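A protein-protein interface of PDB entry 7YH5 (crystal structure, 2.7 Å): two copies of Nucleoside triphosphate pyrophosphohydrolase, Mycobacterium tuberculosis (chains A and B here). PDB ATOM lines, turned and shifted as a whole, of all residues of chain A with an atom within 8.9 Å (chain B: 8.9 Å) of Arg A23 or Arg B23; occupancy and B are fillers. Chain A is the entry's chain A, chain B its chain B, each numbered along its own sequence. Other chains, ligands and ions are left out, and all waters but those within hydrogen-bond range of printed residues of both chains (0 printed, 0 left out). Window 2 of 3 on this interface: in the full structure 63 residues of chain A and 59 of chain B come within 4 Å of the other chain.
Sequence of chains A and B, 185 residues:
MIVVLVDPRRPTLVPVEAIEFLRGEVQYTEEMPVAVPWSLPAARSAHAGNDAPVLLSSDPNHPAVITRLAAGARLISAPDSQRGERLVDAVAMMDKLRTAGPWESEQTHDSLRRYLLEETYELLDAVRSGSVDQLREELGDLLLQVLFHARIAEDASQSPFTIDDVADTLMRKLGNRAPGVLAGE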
ATOM      1  N   VAL A  16      13.787  20.347  12.355  1.00  0.00           N
ATOM      2  CA  VAL A  16      14.974  20.804  11.631  1.00  0.00           C
ATOM      3  C   VAL A  16      15.135  22.315  11.747  1.00  0.00           C
ATOM      4  O   VAL A  16      16.263  22.827  11.767  1.00  0.00           O
ATOM      5  CB  VAL A  16      14.912  20.358  10.155  1.00  0.00           C
ATOM      6  CG1 VAL A  16      16.242  20.594   9.475  1.00  0.00           C
ATOM      7  CG2 VAL A  16      14.546  18.904  10.053  1.00  0.00           C
ATOM      8  N   ALA A  18      14.973  24.086  14.200  1.00  0.00           N
ATOM      9  CA  ALA A  18      15.554  24.466  15.480  1.00  0.00           C
ATOM     10  C   ALA A  18      17.045  24.172  15.577  1.00  0.00           C
ATOM     11  O   ALA A  18      17.653  24.479  16.606  1.00  0.00           O
ATOM     12  CB  ALA A  18      14.818  23.753  16.620  1.00  0.00           C
ATOM     13  N   ILE A  19      17.642  23.576  14.540  1.00  0.00           N
ATOM     14  CA  ILE A  19      19.054  23.201  14.594  1.00  0.00           C
ATOM     15  C   ILE A  19      19.931  24.430  14.812  1.00  0.00           C
ATOM     16  O   ILE A  19      20.902  24.390  15.579  1.00  0.00           O
ATOM     17  CB  ILE A  19      19.448  22.430  13.320  1.00  0.00           C
ATOM     18  CG1 ILE A  19      18.885  21.009  13.377  1.00  0.00           C
ATOM     19  CG2 ILE A  19      20.958  22.390  13.147  1.00  0.00           C
ATOM     20  CD1 ILE A  19      18.992  20.263  12.073  1.00  0.00           C
ATOM     21  N   GLU A  20      19.598  25.542  14.148  1.00  0.00           N
ATOM     22  CA  GLU A  20      20.376  26.770  14.301  1.00  0.00           C
ATOM     23  C   GLU A  20      20.470  27.213  15.756  1.00  0.00           C
ATOM     24  O   GLU A  20      21.461  27.840  16.149  1.00  0.00           O
ATOM     25  CB  GLU A  20      19.757  27.898  13.471  1.00  0.00           C
ATOM     26  CG  GLU A  20      20.111  27.898  11.995  1.00  0.00           C
ATOM     27  CD  GLU A  20      19.467  29.057  11.254  1.00  0.00           C
ATOM     28  OE1 GLU A  20      20.082  29.574  10.297  1.00  0.00           O
ATOM     29  OE2 GLU A  20      18.346  29.454  11.636  1.00  0.00           O
ATOM     30  N   PHE A  21      19.468  26.887  16.570  1.00  0.00           N
ATOM     31  CA  PHE A  21      19.270  27.540  17.855  1.00  0.00           C
ATOM     32  C   PHE A  21      19.690  26.699  19.052  1.00  0.00           C
ATOM     33  O   PHE A  21      19.775  27.236  20.162  1.00  0.00           O
ATOM     34  CB  PHE A  21      17.804  27.956  17.995  1.00  0.00           C
ATOM     35  CG  PHE A  21      17.332  28.836  16.878  1.00  0.00           C
ATOM     36  CD1 PHE A  21      17.883  30.094  16.705  1.00  0.00           C
ATOM     37  CD2 PHE A  21      16.362  28.404  15.990  1.00  0.00           C
ATOM     38  CE1 PHE A  21      17.462  30.916  15.680  1.00  0.00           C
ATOM     39  CE2 PHE A  21      15.938  29.221  14.957  1.00  0.00           C
ATOM     40  CZ  PHE A  21      16.489  30.478  14.803  1.00  0.00           C
ATOM     41  N   LEU A  22      19.939  25.406  18.871  1.00  0.00           N
ATOM     42  CA  LEU A  22      20.372  24.561  19.981  1.00  0.00           C
ATOM     43  C   LEU A  22      21.886  24.481  20.076  1.00  0.00           C
ATOM     44  O   LEU A  22      22.458  23.421  20.348  1.00  0.00           O
ATOM     45  CB  LEU A  22      19.750  23.175  19.849  1.00  0.00           C
ATOM     46  CG  LEU A  22      18.221  23.266  19.847  1.00  0.00           C
ATOM     47  CD1 LEU A  22      17.582  22.214  18.950  1.00  0.00           C
ATOM     48  CD2 LEU A  22      17.671  23.189  21.264  1.00  0.00           C
ATOM     49  N   ARG A  23      22.561  25.605  19.856  1.00  0.00           N
ATOM     50  CA  ARG A  23      24.014  25.670  19.885  1.00  0.00           C
ATOM     51  C   ARG A  23      24.559  26.297  21.161  1.00  0.00           C
ATOM     52  O   ARG A  23      25.572  25.827  21.688  1.00  0.00           O
ATOM     53  CB  ARG A  23      24.530  26.450  18.671  1.00  0.00           C
ATOM     54  N   GLY A  24      23.913  27.340  21.677  1.00  0.00           N
ATOM     55  CA  GLY A  24      24.429  28.050  22.832  1.00  0.00           C
ATOM     56  C   GLY A  24      23.907  27.541  24.160  1.00  0.00           C
ATOM     57  O   GLY A  24      23.843  26.329  24.388  1.00  0.00           O
ATOM     58  N   GLU A  25      23.550  28.459  25.053  1.00  0.00           N
ATOM     59  CA  GLU A  25      22.919  28.070  26.305  1.00  0.00           C
ATOM     60  C   GLU A  25      21.479  27.655  26.043  1.00  0.00           C
ATOM     61  O   GLU A  25      20.752  28.317  25.297  1.00  0.00           O
ATOM     62  CB  GLU A  25      22.961  29.224  27.307  1.00  0.00           C
ATOM     63  CG  GLU A  25      24.275  29.991  27.320  1.00  0.00           C
ATOM     64  CD  GLU A  25      24.206  31.257  28.152  1.00  0.00           C
ATOM     65  OE1 GLU A  25      23.098  31.613  28.609  1.00  0.00           O
ATOM     66  OE2 GLU A  25      25.260  31.896  28.351  1.00  0.00           O
ATOM     67  N   VAL A  26      21.065  26.548  26.653  1.00  0.00           N
ATOM     68  CA  VAL A  26      19.724  26.011  26.453  1.00  0.00           C
ATOM     69  C   VAL A  26      19.209  25.465  27.780  1.00  0.00           C
ATOM     70  O   VAL A  26      19.968  24.897  28.571  1.00  0.00           O
ATOM     71  CB  VAL A  26      19.721  24.935  25.343  1.00  0.00           C
ATOM     72  CG1 VAL A  26      20.846  23.943  25.561  1.00  0.00           C
ATOM     73  CG2 VAL A  26      18.370  24.230  25.248  1.00  0.00           C
ATOM     74  N   TYR A  28      16.038  23.074  29.678  1.00  0.00           N
ATOM     75  CA  TYR A  28      15.102  21.984  29.446  1.00  0.00           C
ATOM     76  C   TYR A  28      14.166  21.848  30.636  1.00  0.00           C
ATOM     77  O   TYR A  28      14.571  22.047  31.785  1.00  0.00           O
ATOM     78  CB  TYR A  28      15.824  20.645  29.221  1.00  0.00           C
ATOM     79  CG  TYR A  28      17.156  20.758  28.518  1.00  0.00           C
ATOM     80  CD1 TYR A  28      18.315  21.046  29.227  1.00  0.00           C
ATOM     81  CD2 TYR A  28      17.258  20.559  27.148  1.00  0.00           C
ATOM     82  CE1 TYR A  28      19.534  21.151  28.590  1.00  0.00           C
ATOM     83  CE2 TYR A  28      18.474  20.657  26.503  1.00  0.00           C
ATOM     84  CZ  TYR A  28      19.610  20.951  27.227  1.00  0.00           C
ATOM     85  OH  TYR A  28      20.823  21.046  26.586  1.00  0.00           O
ATOM     86  N   LEU A  40      23.288  17.111  23.271  1.00  0.00           N
ATOM     87  CA  LEU A  40      23.613  18.427  22.732  1.00  0.00           C
ATOM     88  C   LEU A  40      24.998  18.781  23.260  1.00  0.00           C
ATOM     89  O   LEU A  40      25.161  19.541  24.215  1.00  0.00           O
ATOM     90  CB  LEU A  40      22.560  19.455  23.121  1.00  0.00           C
ATOM     91  CG  LEU A  40      21.150  19.112  22.646  1.00  0.00           C
ATOM     92  CD1 LEU A  40      20.124  19.671  23.604  1.00  0.00           C
ATOM     93  CD2 LEU A  40      20.922  19.638  21.239  1.00  0.00           C
ATOM     94  N   PRO A  41      26.011  18.186  22.616  1.00  0.00           N
ATOM     95  CA  PRO A  41      27.399  18.350  23.043  1.00  0.00           C
ATOM     96  C   PRO A  41      27.754  19.817  23.246  1.00  0.00           C
ATOM     97  O   PRO A  41      28.534  20.158  24.142  1.00  0.00           O
ATOM     98  CB  PRO A  41      28.334  17.706  22.018  1.00  0.00           C
ATOM     99  N   ALA A  42      27.181  20.698  22.428  1.00  0.00           N
ATOM    100  CA  ALA A  42      27.302  22.142  22.616  1.00  0.00           C
ATOM    101  C   ALA A  42      26.265  22.575  23.646  1.00  0.00           C
ATOM    102  O   ALA A  42      25.128  22.915  23.314  1.00  0.00           O
ATOM    103  CB  ALA A  42      27.121  22.874  21.294  1.00  0.00           C
ATOM    104  N   ALA A  43      26.662  22.561  24.914  1.00  0.00           N
ATOM    105  CA  ALA A  43      25.746  22.869  26.007  1.00  0.00           C
ATOM    106  C   ALA A  43      25.880  24.328  26.435  1.00  0.00           C
ATOM    107  O   ALA A  43      26.049  24.627  27.617  1.00  0.00           O
ATOM    108  CB  ALA A  43      25.999  21.943  27.189  1.00  0.00           C
ATOM    109  N   PRO A  53      18.401  31.889  26.439  1.00  0.00           N
ATOM    110  CA  PRO A  53      17.519  32.345  25.352  1.00  0.00           C
ATOM    111  C   PRO A  53      16.674  31.236  24.753  1.00  0.00           C
ATOM    112  O   PRO A  53      15.605  31.524  24.202  1.00  0.00           O
ATOM    113  CB  PRO A  53      18.500  32.918  24.320  1.00  0.00           C
ATOM    114  CG  PRO A  53      19.796  32.233  24.610  1.00  0.00           C
ATOM    115  CD  PRO A  53      19.825  32.026  26.095  1.00  0.00           C
ATOM    116  N   VAL A  54      17.117  29.985  24.835  1.00  0.00           N
ATOM    117  CA  VAL A  54      16.475  28.866  24.155  1.00  0.00           C
ATOM    118  C   VAL A  54      15.970  27.892  25.205  1.00  0.00           C
ATOM    119  O   VAL A  54      16.746  27.418  26.045  1.00  0.00           O
ATOM    120  CB  VAL A  54      17.434  28.164  23.181  1.00  0.00           C
ATOM    121  CG1 VAL A  54      16.719  27.027  22.464  1.00  0.00           C
ATOM    122  CG2 VAL A  54      18.009  29.168  22.188  1.00  0.00           C
ATOM    123  N   ALA B  18      22.190  14.102  16.067  1.00  0.00           N
ATOM    124  CA  ALA B  18      22.691  14.367  14.725  1.00  0.00           C
ATOM    125  C   ALA B  18      22.877  15.847  14.415  1.00  0.00           C
ATOM    126  O   ALA B  18      23.461  16.169  13.374  1.00  0.00           O
ATOM    127  CB  ALA B  18      21.749  13.753  13.679  1.00  0.00           C
ATOM    128  N   ILE B  19      22.419  16.752  15.285  1.00  0.00           N
ATOM    129  CA  ILE B  19      22.335  18.158  14.897  1.00  0.00           C
ATOM    130  C   ILE B  19      23.718  18.765  14.667  1.00  0.00           C
ATOM    131  O   ILE B  19      23.871  19.653  13.819  1.00  0.00           O
ATOM    132  CB  ILE B  19      21.521  18.964  15.931  1.00  0.00           C
ATOM    133  CG1 ILE B  19      22.392  19.409  17.107  1.00  0.00           C
ATOM    134  CG2 ILE B  19      20.324  18.161  16.421  1.00  0.00           C
ATOM    135  CD1 ILE B  19      21.884  20.657  17.790  1.00  0.00           C
ATOM    136  N   GLU B  20      24.746  18.305  15.388  1.00  0.00           N
ATOM    137  CA  GLU B  20      26.088  18.832  15.149  1.00  0.00           C
ATOM    138  C   GLU B  20      26.620  18.380  13.796  1.00  0.00           C
ATOM    139  O   GLU B  20      27.322  19.133  13.112  1.00  0.00           O
ATOM    140  CB  GLU B  20      27.042  18.408  16.265  1.00  0.00           C
ATOM    141  CG  GLU B  20      26.819  19.135  17.573  1.00  0.00           C
ATOM    142  CD  GLU B  20      26.916  20.637  17.421  1.00  0.00           C
ATOM    143  OE1 GLU B  20      27.874  21.112  16.776  1.00  0.00           O
ATOM    144  OE2 GLU B  20      26.024  21.345  17.935  1.00  0.00           O
ATOM    145  N   PHE B  21      26.295  17.157  13.395  1.00  0.00           N
ATOM    146  CA  PHE B  21      26.694  16.645  12.094  1.00  0.00           C
ATOM    147  C   PHE B  21      25.813  17.156  10.962  1.00  0.00           C
ATOM    148  O   PHE B  21      26.092  16.851   9.798  1.00  0.00           O
ATOM    149  CB  PHE B  21      26.683  15.115  12.118  1.00  0.00           C
ATOM    150  CG  PHE B  21      27.524  14.524  13.214  1.00  0.00           C
ATOM    151  CD1 PHE B  21      28.906  14.524  13.117  1.00  0.00           C
ATOM    152  CD2 PHE B  21      26.935  13.977  14.343  1.00  0.00           C
ATOM    153  CE1 PHE B  21      29.685  13.982  14.118  1.00  0.00           C
ATOM    154  CE2 PHE B  21      27.711  13.435  15.350  1.00  0.00           C
ATOM    155  CZ  PHE B  21      29.089  13.438  15.238  1.00  0.00           C
ATOM    156  N   LEU B  22      24.771  17.930  11.264  1.00  0.00           N
ATOM    157  CA  LEU B  22      23.833  18.402  10.254  1.00  0.00           C
ATOM    158  C   LEU B  22      24.082  19.840   9.815  1.00  0.00           C
ATOM    159  O   LEU B  22      23.403  20.312   8.898  1.00  0.00           O
ATOM    160  CB  LEU B  22      22.394  18.274  10.763  1.00  0.00           C
ATOM    161  CG  LEU B  22      21.804  16.867  10.869  1.00  0.00           C
ATOM    162  CD1 LEU B  22      20.354  16.942  11.311  1.00  0.00           C
ATOM    163  CD2 LEU B  22      21.935  16.108   9.557  1.00  0.00           C
ATOM    164  N   ARG B  23      25.022  20.550  10.441  1.00  0.00           N
ATOM    165  CA  ARG B  23      25.290  21.932  10.059  1.00  0.00           C
ATOM    166  C   ARG B  23      26.396  22.061   9.020  1.00  0.00           C
ATOM    167  O   ARG B  23      26.621  23.166   8.512  1.00  0.00           O
ATOM    168  CB  ARG B  23      25.652  22.779  11.293  1.00  0.00           C
ATOM    169  CG  ARG B  23      26.456  22.066  12.363  1.00  0.00           C
ATOM    170  CD  ARG B  23      26.737  22.997  13.535  1.00  0.00           C
ATOM    171  NE  ARG B  23      25.520  23.654  14.006  1.00  0.00           N
ATOM    172  CZ  ARG B  23      25.152  23.736  15.281  1.00  0.00           C
ATOM    173  NH1 ARG B  23      25.912  23.210  16.231  1.00  0.00           N
ATOM    174  NH2 ARG B  23      24.024  24.352  15.610  1.00  0.00           N
ATOM    175  N   GLY B  24      27.085  20.976   8.695  1.00  0.00           N
ATOM    176  CA  GLY B  24      28.082  20.976   7.648  1.00  0.00           C
ATOM    177  C   GLY B  24      27.495  20.560   6.316  1.00  0.00           C
ATOM    178  O   GLY B  24      26.291  20.669   6.073  1.00  0.00           O
ATOM    179  N   GLU B  25      28.370  20.074   5.440  1.00  0.00           N
ATOM    180  CA  GLU B  25      27.939  19.547   4.152  1.00  0.00           C
ATOM    181  C   GLU B  25      27.162  18.254   4.363  1.00  0.00           C
ATOM    182  O   GLU B  25      27.708  17.272   4.877  1.00  0.00           O
ATOM    183  CB  GLU B  25      29.151  19.308   3.255  1.00  0.00           C
ATOM    184  CG  GLU B  25      28.852  18.557   1.966  1.00  0.00           C
ATOM    185  CD  GLU B  25      30.070  18.446   1.067  1.00  0.00           C
ATOM    186  OE1 GLU B  25      30.959  19.319   1.162  1.00  0.00           O
ATOM    187  OE2 GLU B  25      30.140  17.488   0.267  1.00  0.00           O
ATOM    188  N   VAL B  26      25.882  18.256   3.984  1.00  0.00           N
ATOM    189  CA  VAL B  26      25.043  17.070   4.082  1.00  0.00           C
ATOM    190  C   VAL B  26      24.316  16.884   2.756  1.00  0.00           C
ATOM    191  O   VAL B  26      24.090  17.834   2.001  1.00  0.00           O
ATOM    192  CB  VAL B  26      24.023  17.152   5.245  1.00  0.00           C
ATOM    193  CG1 VAL B  26      24.672  17.724   6.508  1.00  0.00           C
ATOM    194  CG2 VAL B  26      22.782  17.938   4.838  1.00  0.00           C
ATOM    195  N   SER B  39      15.824  24.491   5.786  1.00  0.00           N
ATOM    196  CA  SER B  39      16.314  24.631   7.151  1.00  0.00           C
ATOM    197  C   SER B  39      17.797  24.316   7.273  1.00  0.00           C
ATOM    198  O   SER B  39      18.516  25.014   7.993  1.00  0.00           O
ATOM    199  CB  SER B  39      15.519  23.725   8.093  1.00  0.00           C
ATOM    200  OG  SER B  39      14.130  23.995   8.015  1.00  0.00           O
ATOM    201  N   LEU B  40      18.271  23.281   6.587  1.00  0.00           N
ATOM    202  CA  LEU B  40      19.698  22.998   6.547  1.00  0.00           C
ATOM    203  C   LEU B  40      20.356  23.983   5.591  1.00  0.00           C
ATOM    204  O   LEU B  40      20.074  23.963   4.386  1.00  0.00           O
ATOM    205  CB  LEU B  40      19.957  21.553   6.119  1.00  0.00           C
ATOM    206  CG  LEU B  40      19.383  20.499   7.069  1.00  0.00           C
ATOM    207  CD1 LEU B  40      19.951  19.120   6.778  1.00  0.00           C
ATOM    208  CD2 LEU B  40      19.654  20.893   8.511  1.00  0.00           C
ATOM    209  N   PRO B  41      21.229  24.860   6.091  1.00  0.00           N
ATOM    210  CA  PRO B  41      21.791  25.903   5.215  1.00  0.00           C
ATOM    211  C   PRO B  41      22.600  25.344   4.058  1.00  0.00           C
ATOM    212  O   PRO B  41      22.309  25.651   2.895  1.00  0.00           O
ATOM    213  CB  PRO B  41      22.654  26.731   6.180  1.00  0.00           C
ATOM    214  CG  PRO B  41      23.001  25.780   7.288  1.00  0.00           C
ATOM    215  CD  PRO B  41      21.800  24.899   7.448  1.00  0.00           C
ATOM    216  N   ALA B  42      23.596  24.508   4.350  1.00  0.00           N
ATOM    217  CA  ALA B  42      24.528  24.017   3.341  1.00  0.00           C
ATOM    218  C   ALA B  42      24.270  22.561   2.970  1.00  0.00           C
ATOM    219  O   ALA B  42      25.195  21.743   2.969  1.00  0.00           O
ATOM    220  CB  ALA B  42      25.967  24.182   3.834  1.00  0.00           C
ATOM    221  N   ALA B  43      23.026  22.233   2.638  1.00  0.00           N
ATOM    222  CA  ALA B  43      22.646  20.893   2.223  1.00  0.00           C
ATOM    223  C   ALA B  43      22.381  20.869   0.723  1.00  0.00           C
ATOM    224  O   ALA B  43      22.210  21.910   0.084  1.00  0.00           O
ATOM    225  CB  ALA B  43      21.405  20.419   2.981  1.00  0.00           C
ATOM    226  N   VAL B  54      27.940  13.219   5.405  1.00  0.00           N
ATOM    227  CA  VAL B  54      26.724  12.783   6.079  1.00  0.00           C
ATOM    228  C   VAL B  54      25.569  12.855   5.090  1.00  0.00           C
ATOM    229  O   VAL B  54      25.428  13.841   4.361  1.00  0.00           O
ATOM    230  CB  VAL B  54      26.431  13.618   7.342  1.00  0.00           C
ATOM    231  CG1 VAL B  54      26.584  15.090   7.059  1.00  0.00           C
ATOM    232  CG2 VAL B  54      25.035  13.311   7.867  1.00  0.00           C
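The backbone carbonyl oxygen (O) of Ile A19 is in hydrogen-bond range of the guanidinium group (NH2) of Arg B23, at 3.1 Å.
The side-chain carboxylate (OE2) of Glu B20 lies within salt-bridge range of the guanidinium group (NH1) of Arg B23, at 2.5 Å.
Among the printed residues, pairs that only touch across the chains: Val A16 with Ser B39 (3.5 Å), Val A16 with Leu B40 (3.6 Å), Ile A19 with Leu B22 (3.7 Å), Ile A19 with Leu B40 (3.7 Å), Leu A40 with Ile B19 (3.7 Å), Arg A23 with Arg B23 (3.7 Å), Leu A22 with Ile B19 (3.8 Å) and Ala A42 with Glu B20 (3.9 Å).
Arg A23 touches one residue of chain B.
No residue of chain B comes within 4 Å of Gly A24.
Printed residues of chain A within 4 Å of Ile B19: Leu A22 (3.8 Å) and Leu A40 (3.7 Å).
Of the printed residues of chain B, Leu A40 touches Ile B19 (3.7 Å).
Of the printed residues of chain A, Leu B40 touches Val A16 and Ile A19.
Of the printed residues of chain A, Glu B20 touches Ala A42 (3.9 Å).
The nearest residue of chain A that does not touch Arg B23 is Glu A20 (4.4 Å).
The nearest printed residue of chain B that does not touch Leu A40 is Glu B20 (6.0 Å).
Of the 17 printed residues of chain A, 6 touch a printed residue of chain B.
Hydrophobic or aromatic side chains of chain A that line the printed part of chain B: Val A16, Ile A19, Leu A22, Leu A40 and Ala A42.
Of the 15 printed residues of chain B, 6 touch a printed residue of chain A.
Printed residues of chain B that touch a printed residue of chain A: Ile B19, Glu B20, Leu B22, Arg B23, Ser B39 and Leu B40.
Among the printed residues, 9 pairs touch across the chains.
Ile A19 touches Leu B22, and with the chains exchanged Leu A22 touches Ile B19.
Ile A19 touches Arg B23, but with the chains exchanged Arg A23 does not touch Ile B19 (5.4 Å).
Arg B23 touches its own counterpart, Arg A23.
Ala A42 touches Glu B20, but with the chains exchanged Glu A20 does not touch Ala B42 (8.6 Å).
Positions printed for both chains: 18, 19, 20, 21, 22, 23, 24, 25, 26, 40, 41, 42, 43 and 54.
Of the 9 pairs that touch across the chains among the printed residues, 5 have their exchanged pair printed and touching as well.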
